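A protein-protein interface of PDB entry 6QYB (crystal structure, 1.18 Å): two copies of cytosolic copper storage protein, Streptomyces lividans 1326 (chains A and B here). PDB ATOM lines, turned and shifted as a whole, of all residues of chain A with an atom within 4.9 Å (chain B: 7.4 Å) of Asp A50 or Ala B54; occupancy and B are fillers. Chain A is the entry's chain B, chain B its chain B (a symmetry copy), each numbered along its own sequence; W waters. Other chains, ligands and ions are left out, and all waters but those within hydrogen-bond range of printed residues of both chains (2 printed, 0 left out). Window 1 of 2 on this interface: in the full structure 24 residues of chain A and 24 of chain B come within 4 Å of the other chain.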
ATOM      1  N   MET A  46      14.686 -16.151 -12.263  1.00  0.00           N
ATOM      2  CA  MET A  46      15.086 -16.762 -10.970  1.00  0.00           C
ATOM      3  C   MET A  46      14.780 -15.786  -9.834  1.00  0.00           C
ATOM      4  O   MET A  46      14.205 -16.201  -8.834  1.00  0.00           O
ATOM      5  CB  MET A  46      16.571 -17.126 -10.942  1.00  0.00           C
ATOM      6  CG  MET A  46      16.931 -18.156 -11.973  1.00  0.00           C
ATOM      7  SD  MET A  46      18.672 -18.629 -11.909  1.00  0.00           S
ATOM      8  CE  MET A  46      19.578 -17.120 -12.192  1.00  0.00           C
ATOM      9  N   ASP A  47      15.137 -14.512 -10.001  1.00  0.00           N
ATOM     10  CA  ASP A  47      14.858 -13.501  -8.952  1.00  0.00           C
ATOM     11  C   ASP A  47      13.338 -13.386  -8.773  1.00  0.00           C
ATOM     12  O   ASP A  47      12.847 -13.306  -7.643  1.00  0.00           O
ATOM     13  CB  ASP A  47      15.399 -12.116  -9.327  1.00  0.00           C
ATOM     14  CG  ASP A  47      16.906 -11.974  -9.304  1.00  0.00           C
ATOM     15  OD1 ASP A  47      17.596 -12.896  -8.798  1.00  0.00           O
ATOM     16  OD2 ASP A  47      17.371 -10.929  -9.829  1.00  0.00           O
ATOM     17  N   CYS A  48      12.612 -13.334  -9.878  1.00  0.00           N
ATOM     18  CA  CYS A  48      11.152 -13.096  -9.831  1.00  0.00           C
ATOM     19  C   CYS A  48      10.474 -14.251  -9.085  1.00  0.00           C
ATOM     20  O   CYS A  48       9.564 -14.019  -8.269  1.00  0.00           O
ATOM     21  CB  CYS A  48      10.570 -12.928 -11.227  1.00  0.00           C
ATOM     22  SG  CYS A  48       9.083 -11.940 -11.164  1.00  0.00           S
ATOM     23  N   ALA A  49      10.948 -15.476  -9.311  1.00  0.00           N
ATOM     24  CA  ALA A  49      10.400 -16.663  -8.626  1.00  0.00           C
ATOM     25  C   ALA A  49      10.697 -16.543  -7.131  1.00  0.00           C
ATOM     26  O   ALA A  49       9.798 -16.755  -6.318  1.00  0.00           O
ATOM     27  CB  ALA A  49      10.964 -17.932  -9.214  1.00  0.00           C
ATOM     28  N   ASP A  50      11.938 -16.211  -6.771  1.00  0.00           N
ATOM     29  CA  ASP A  50      12.292 -16.147  -5.336  1.00  0.00           C
ATOM     30  C   ASP A  50      11.487 -15.061  -4.612  1.00  0.00           C
ATOM     31  O   ASP A  50      11.012 -15.292  -3.499  1.00  0.00           O
ATOM     32  CB  ASP A  50      13.786 -15.895  -5.207  1.00  0.00           C
ATOM     33  CG  ASP A  50      14.631 -17.103  -5.572  1.00  0.00           C
ATOM     34  OD1 ASP A  50      14.107 -18.236  -5.539  1.00  0.00           O
ATOM     35  OD2 ASP A  50      15.756 -16.892  -5.972  1.00  0.00           O
ATOM     36  N   VAL A  51      11.333 -13.900  -5.223  1.00  0.00           N
ATOM     37  CA  VAL A  51      10.637 -12.793  -4.527  1.00  0.00           C
ATOM     38  C   VAL A  51       9.127 -13.065  -4.487  1.00  0.00           C
ATOM     39  O   VAL A  51       8.521 -12.818  -3.425  1.00  0.00           O
ATOM     40  CB  VAL A  51      10.978 -11.446  -5.182  1.00  0.00           C
ATOM     41  CG1 VAL A  51      10.144 -10.314  -4.606  1.00  0.00           C
ATOM     42  CG2 VAL A  51      12.476 -11.145  -5.046  1.00  0.00           C
ATOM     43  N   CYS A  52       8.541 -13.640  -5.542  1.00  0.00           N
ATOM     44  CA  CYS A  52       7.093 -13.980  -5.544  1.00  0.00           C
ATOM     45  C   CYS A  52       6.851 -15.059  -4.480  1.00  0.00           C
ATOM     46  O   CYS A  52       5.822 -14.982  -3.767  1.00  0.00           O
ATOM     47  CB  CYS A  52       6.640 -14.448  -6.921  1.00  0.00           C
ATOM     48  SG  CYS A  52       6.331 -13.100  -8.093  1.00  0.00           S
ATOM     49  N   THR A  53       7.771 -16.013  -4.317  1.00  0.00           N
ATOM     50  CA  THR A  53       7.593 -17.075  -3.299  1.00  0.00           C
ATOM     51  C   THR A  53       7.558 -16.439  -1.903  1.00  0.00           C
ATOM     52  O   THR A  53       6.704 -16.755  -1.087  1.00  0.00           O
ATOM     53  CB  THR A  53       8.720 -18.096  -3.440  1.00  0.00           C
ATOM     54  OG1 THR A  53       8.537 -18.759  -4.688  1.00  0.00           O
ATOM     55  CG2 THR A  53       8.752 -19.093  -2.304  1.00  0.00           C
ATOM     56  N   ALA A  54       8.501 -15.550  -1.614  1.00  0.00           N
ATOM     57  CA  ALA A  54       8.573 -14.899  -0.291  1.00  0.00           C
ATOM     58  C   ALA A  54       7.336 -14.028  -0.076  1.00  0.00           C
ATOM     59  O   ALA A  54       6.783 -14.034   1.030  1.00  0.00           O
ATOM     60  CB  ALA A  54       9.837 -14.093  -0.183  1.00  0.00           C
ATOM     61  N   CYS B  15      22.502 -12.704   5.422  1.00  0.00           N
ATOM     62  CA  CYS B  15      21.130 -13.139   5.056  1.00  0.00           C
ATOM     63  C   CYS B  15      20.994 -14.625   5.398  1.00  0.00           C
ATOM     64  O   CYS B  15      19.950 -15.034   5.969  1.00  0.00           O
ATOM     65  CB  CYS B  15      20.810 -12.936   3.581  1.00  0.00           C
ATOM     66  SG  CYS B  15      20.391 -11.235   3.156  1.00  0.00           S
ATOM     67  N   ALA B  19      18.467 -15.836   8.212  1.00  0.00           N
ATOM     68  CA  ALA B  19      17.339 -16.712   7.801  1.00  0.00           C
ATOM     69  C   ALA B  19      17.267 -17.902   8.757  1.00  0.00           C
ATOM     70  O   ALA B  19      16.193 -18.187   9.325  1.00  0.00           O
ATOM     71  CB  ALA B  19      17.498 -17.136   6.372  1.00  0.00           C
ATOM     72  N   CYS B  48      10.930 -12.887   8.313  1.00  0.00           N
ATOM     73  CA  CYS B  48      12.354 -12.490   8.247  1.00  0.00           C
ATOM     74  C   CYS B  48      13.160 -13.605   7.568  1.00  0.00           C
ATOM     75  O   CYS B  48      14.040 -13.320   6.737  1.00  0.00           O
ATOM     76  CB  CYS B  48      12.908 -12.176   9.629  1.00  0.00           C
ATOM     77  SG  CYS B  48      14.276 -11.033   9.502  1.00  0.00           S
ATOM     78  N   ALA B  49      12.825 -14.859   7.868  1.00  0.00           N
ATOM     79  CA  ALA B  49      13.505 -16.015   7.253  1.00  0.00           C
ATOM     80  C   ALA B  49      13.201 -16.019   5.755  1.00  0.00           C
ATOM     81  O   ALA B  49      14.121 -16.176   4.953  1.00  0.00           O
ATOM     82  CB  ALA B  49      13.085 -17.303   7.917  1.00  0.00           C
ATOM     83  N   ASP B  50      11.932 -15.850   5.380  1.00  0.00           N
ATOM     84  CA  ASP B  50      11.578 -15.911   3.944  1.00  0.00           C
ATOM     85  C   ASP B  50      12.258 -14.787   3.155  1.00  0.00           C
ATOM     86  O   ASP B  50      12.761 -15.029   2.056  1.00  0.00           O
ATOM     87  CB  ASP B  50      10.066 -15.837   3.806  1.00  0.00           C
ATOM     88  CG  ASP B  50       9.360 -17.108   4.245  1.00  0.00           C
ATOM     89  OD1 ASP B  50      10.008 -18.175   4.277  1.00  0.00           O
ATOM     90  OD2 ASP B  50       8.217 -17.001   4.635  1.00  0.00           O
ATOM     91  N   VAL B  51      12.279 -13.581   3.695  1.00  0.00           N
ATOM     92  CA  VAL B  51      12.850 -12.446   2.933  1.00  0.00           C
ATOM     93  C   VAL B  51      14.381 -12.549   2.903  1.00  0.00           C
ATOM     94  O   VAL B  51      14.959 -12.299   1.827  1.00  0.00           O
ATOM     95  CB  VAL B  51      12.357 -11.110   3.508  1.00  0.00           C
ATOM     96  CG1 VAL B  51      13.061  -9.927   2.863  1.00  0.00           C
ATOM     97  CG2 VAL B  51      10.835 -10.988   3.359  1.00  0.00           C
ATOM     98  N   CYS B  52      15.023 -12.992   3.989  1.00  0.00           N
ATOM     99  CA  CYS B  52      16.501 -13.167   4.007  1.00  0.00           C
ATOM    100  C   CYS B  52      16.866 -14.272   3.007  1.00  0.00           C
ATOM    101  O   CYS B  52      17.881 -14.123   2.288  1.00  0.00           O
ATOM    102  CB  CYS B  52      16.998 -13.498   5.407  1.00  0.00           C
ATOM    103  SG  CYS B  52      17.151 -12.057   6.497  1.00  0.00           S
ATOM    104  N   THR B  53      16.059 -15.332   2.904  1.00  0.00           N
ATOM    105  CA  THR B  53      16.358 -16.425   1.950  1.00  0.00           C
ATOM    106  C   THR B  53      16.326 -15.874   0.519  1.00  0.00           C
ATOM    107  O   THR B  53      17.213 -16.140  -0.280  1.00  0.00           O
ATOM    108  CB  THR B  53      15.352 -17.556   2.155  1.00  0.00           C
ATOM    109  OG1 THR B  53      15.605 -18.120   3.440  1.00  0.00           O
ATOM    110  CG2 THR B  53      15.436 -18.616   1.081  1.00  0.00           C
ATOM    111  N   ALA B  54      15.291 -15.114   0.181  1.00  0.00           N
ATOM    112  CA  ALA B  54      15.151 -14.555  -1.178  1.00  0.00           C
ATOM    113  C   ALA B  54      16.283 -13.566  -1.448  1.00  0.00           C
ATOM    114  O   ALA B  54      16.837 -13.575  -2.554  1.00  0.00           O
ATOM    115  CB  ALA B  54      13.805 -13.904  -1.329  1.00  0.00           C
ATOM    116  N   THR B  55      16.595 -12.722  -0.473  1.00  0.00           N
ATOM    117  CA  THR B  55      17.600 -11.658  -0.647  1.00  0.00           C
ATOM    118  C   THR B  55      18.963 -12.326  -0.897  1.00  0.00           C
ATOM    119  O   THR B  55      19.691 -11.877  -1.799  1.00  0.00           O
ATOM    120  CB  THR B  55      17.598 -10.721   0.567  1.00  0.00           C
ATOM    121  OG1 THR B  55      16.310 -10.124   0.667  1.00  0.00           O
ATOM    122  CG2 THR B  55      18.657  -9.639   0.478  1.00  0.00           C
ATOM    123  N   ALA B  56      19.332 -13.356  -0.129  1.00  0.00           N
ATOM    124  CA  ALA B  56      20.630 -14.037  -0.319  1.00  0.00           C
ATOM    125  C   ALA B  56      20.734 -14.547  -1.759  1.00  0.00           C
ATOM    126  O   ALA B  56      21.818 -14.467  -2.367  1.00  0.00           O
ATOM    127  CB  ALA B  56      20.767 -15.169   0.662  1.00  0.00           C
ATOM    128  N   ALA B  57      19.636 -15.085  -2.300  1.00  0.00           N
ATOM    129  CA  ALA B  57      19.629 -15.645  -3.666  1.00  0.00           C
ATOM    130  C   ALA B  57      19.786 -14.520  -4.692  1.00  0.00           C
ATOM    131  O   ALA B  57      20.596 -14.619  -5.613  1.00  0.00           O
ATOM    132  CB  ALA B  57      18.394 -16.477  -3.875  1.00  0.00           C
ATOM    133  N   VAL B  58      18.990 -13.466  -4.555  1.00  0.00           N
ATOM    134  CA  VAL B  58      19.039 -12.349  -5.541  1.00  0.00           C
ATOM    135  C   VAL B  58      20.449 -11.744  -5.542  1.00  0.00           C
ATOM    136  O   VAL B  58      20.999 -11.501  -6.621  1.00  0.00           O
ATOM    137  CB  VAL B  58      17.940 -11.320  -5.252  1.00  0.00           C
ATOM    138  CG1 VAL B  58      18.090 -10.054  -6.084  1.00  0.00           C
ATOM    139  CG2 VAL B  58      16.560 -11.941  -5.452  1.00  0.00           C
ATOM    140  N   LEU B  59      21.031 -11.554  -4.360  1.00  0.00           N
ATOM    141  CA  LEU B  59      22.344 -10.861  -4.240  1.00  0.00           C
ATOM    142  C   LEU B  59      23.476 -11.781  -4.718  1.00  0.00           C
ATOM    143  O   LEU B  59      24.544 -11.266  -5.092  1.00  0.00           O
ATOM    144  CB  LEU B  59      22.545 -10.392  -2.795  1.00  0.00           C
ATOM    145  CG  LEU B  59      21.982  -9.004  -2.475  1.00  0.00           C
ATOM    146  CD1 LEU B  59      22.807  -7.924  -3.135  1.00  0.00           C
ATOM    147  CD2 LEU B  59      20.535  -8.830  -2.906  1.00  0.00           C
ATOM    148  N   SER B  60      23.236 -13.083  -4.777  1.00  0.00           N
ATOM    149  CA  SER B  60      24.233 -14.088  -5.226  1.00  0.00           C
ATOM    150  C   SER B  60      24.366 -14.102  -6.755  1.00  0.00           C
ATOM    151  O   SER B  60      25.259 -14.810  -7.256  1.00  0.00           O
ATOM    152  CB  SER B  60      23.884 -15.455  -4.705  1.00  0.00           C
ATOM    153  OG  SER B  60      24.117 -15.544  -3.304  1.00  0.00           O
ATOM    154  N   ARG B  61      23.457 -13.446  -7.484  1.00  0.00           N
ATOM    155  CA  ARG B  61      23.420 -13.500  -8.969  1.00  0.00           C
ATOM    156  C   ARG B  61      23.934 -12.177  -9.542  1.00  0.00           C
ATOM    157  O   ARG B  61      23.470 -11.113  -9.101  1.00  0.00           O
ATOM    158  CB  ARG B  61      21.994 -13.776  -9.457  1.00  0.00           C
ATOM    159  CG  ARG B  61      21.387 -15.051  -8.893  1.00  0.00           C
ATOM    160  CD  ARG B  61      19.945 -15.184  -9.325  1.00  0.00           C
ATOM    161  NE  ARG B  61      19.413 -16.413  -8.777  1.00  0.00           N
ATOM    162  CZ  ARG B  61      18.350 -16.538  -7.983  1.00  0.00           C
ATOM    163  NH1 ARG B  61      17.580 -15.502  -7.683  1.00  0.00           N
ATOM    164  NH2 ARG B  61      18.041 -17.730  -7.509  1.00  0.00           N
ATOM    165  N   VAL B  73      14.813  -5.122  -3.150  1.00  0.00           N
ATOM    166  CA  VAL B  73      14.917  -6.378  -2.357  1.00  0.00           C
ATOM    167  C   VAL B  73      15.725  -6.071  -1.084  1.00  0.00           C
ATOM    168  O   VAL B  73      15.293  -6.461  -0.006  1.00  0.00           O
ATOM    169  CB  VAL B  73      15.546  -7.504  -3.190  1.00  0.00           C
ATOM    170  CG1 VAL B  73      15.924  -8.694  -2.331  1.00  0.00           C
ATOM    171  CG2 VAL B  73      14.635  -7.951  -4.322  1.00  0.00           C
ATOM    172  N   CYS B  77      14.529  -6.361   2.840  1.00  0.00           N
ATOM    173  CA  CYS B  77      15.242  -7.173   3.844  1.00  0.00           C
ATOM    174  C   CYS B  77      15.685  -6.294   5.024  1.00  0.00           C
ATOM    175  O   CYS B  77      15.576  -6.747   6.173  1.00  0.00           O
ATOM    176  CB  CYS B  77      16.402  -7.933   3.235  1.00  0.00           C
ATOM    177  SG  CYS B  77      16.756  -9.404   4.212  1.00  0.00           S
HETATM  178  O   HOH W   1      16.630 -19.415  -4.832  1.00  0.00           O
HETATM  179  O   HOH W   2      21.082 -18.646  -9.566  1.00  0.00           O
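The side-chain carboxylate of Asp A47 is in salt-bridge range of the guanidinium group of Arg B61 (2.8 Å).
The guanidinium group of Arg B61 lies within salt-bridge range of the side-chain carboxylate of Asp A50, 2.9 Å away.
Among the printed residues, pairs that only touch across the chains: Met A46 with Arg B61 (3.5 Å), Asp A47 with Val B58 (3.6 Å), Asp A50 with Ala B54 (3.8 Å), Asp A50 with Ala B57 (3.4 Å), Val A51 with Val B73 (3.9 Å) and Ala A54 with Asp B50 (3.8 Å).
Of the printed residues of chain B, Met A46 touches Arg B61.
Printed residues of chain B within 4 Å of Asp A47: Val B58 (3.6 Å) and Arg B61 (2.8 Å).
Of the printed residues of chain B, Ala A54 touches Asp B50 (3.8 Å).
Thr B53 touches none of the printed residues of chain A.
Of chain A, only Asp A50 (3.8 Å) comes within 4 Å of Ala B54.
Printed residues of chain A within 4 Å of Val B58: Asp A47.
The nearest residue of chain B that does not touch Asp A50 is Val B58 (4.8 Å).
The nearest printed residue of chain A that does not touch Ala B57 is Asp A47 (4.7 Å).
Printed residues of chain B that touch a printed residue of chain A: Asp B50, Ala B54, Ala B57, Val B58, Arg B61 and Val B73.
Hydrophobic or aromatic side chains of chain B within 4 Å of the printed part of chain A: Ala B54, Ala B57, Val B58 and Val B73.
Of the 9 printed residues of chain A, 5 touch a printed residue of chain B.
Among the printed residues, 8 pairs touch across the chains.
Among the printed residues, Asp or Glu carboxylates within 4 Å of a Lys or Arg side-chain nitrogen of the other chain: Asp A47 with Arg B61 (2.8 Å) and Asp A50 with Arg B61 (2.9 Å).
Asp A50 touches Ala B54, and with the chains exchanged Ala A54 touches Asp B50.
Water W1 bridges the side-chain carboxylate of Asp A50 (2.9 Å) and the guanidinium group of Arg B61 (3.5 Å).
Water W2 lies within hydrogen-bond range of NE of Arg B61 and SD of Met A46.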
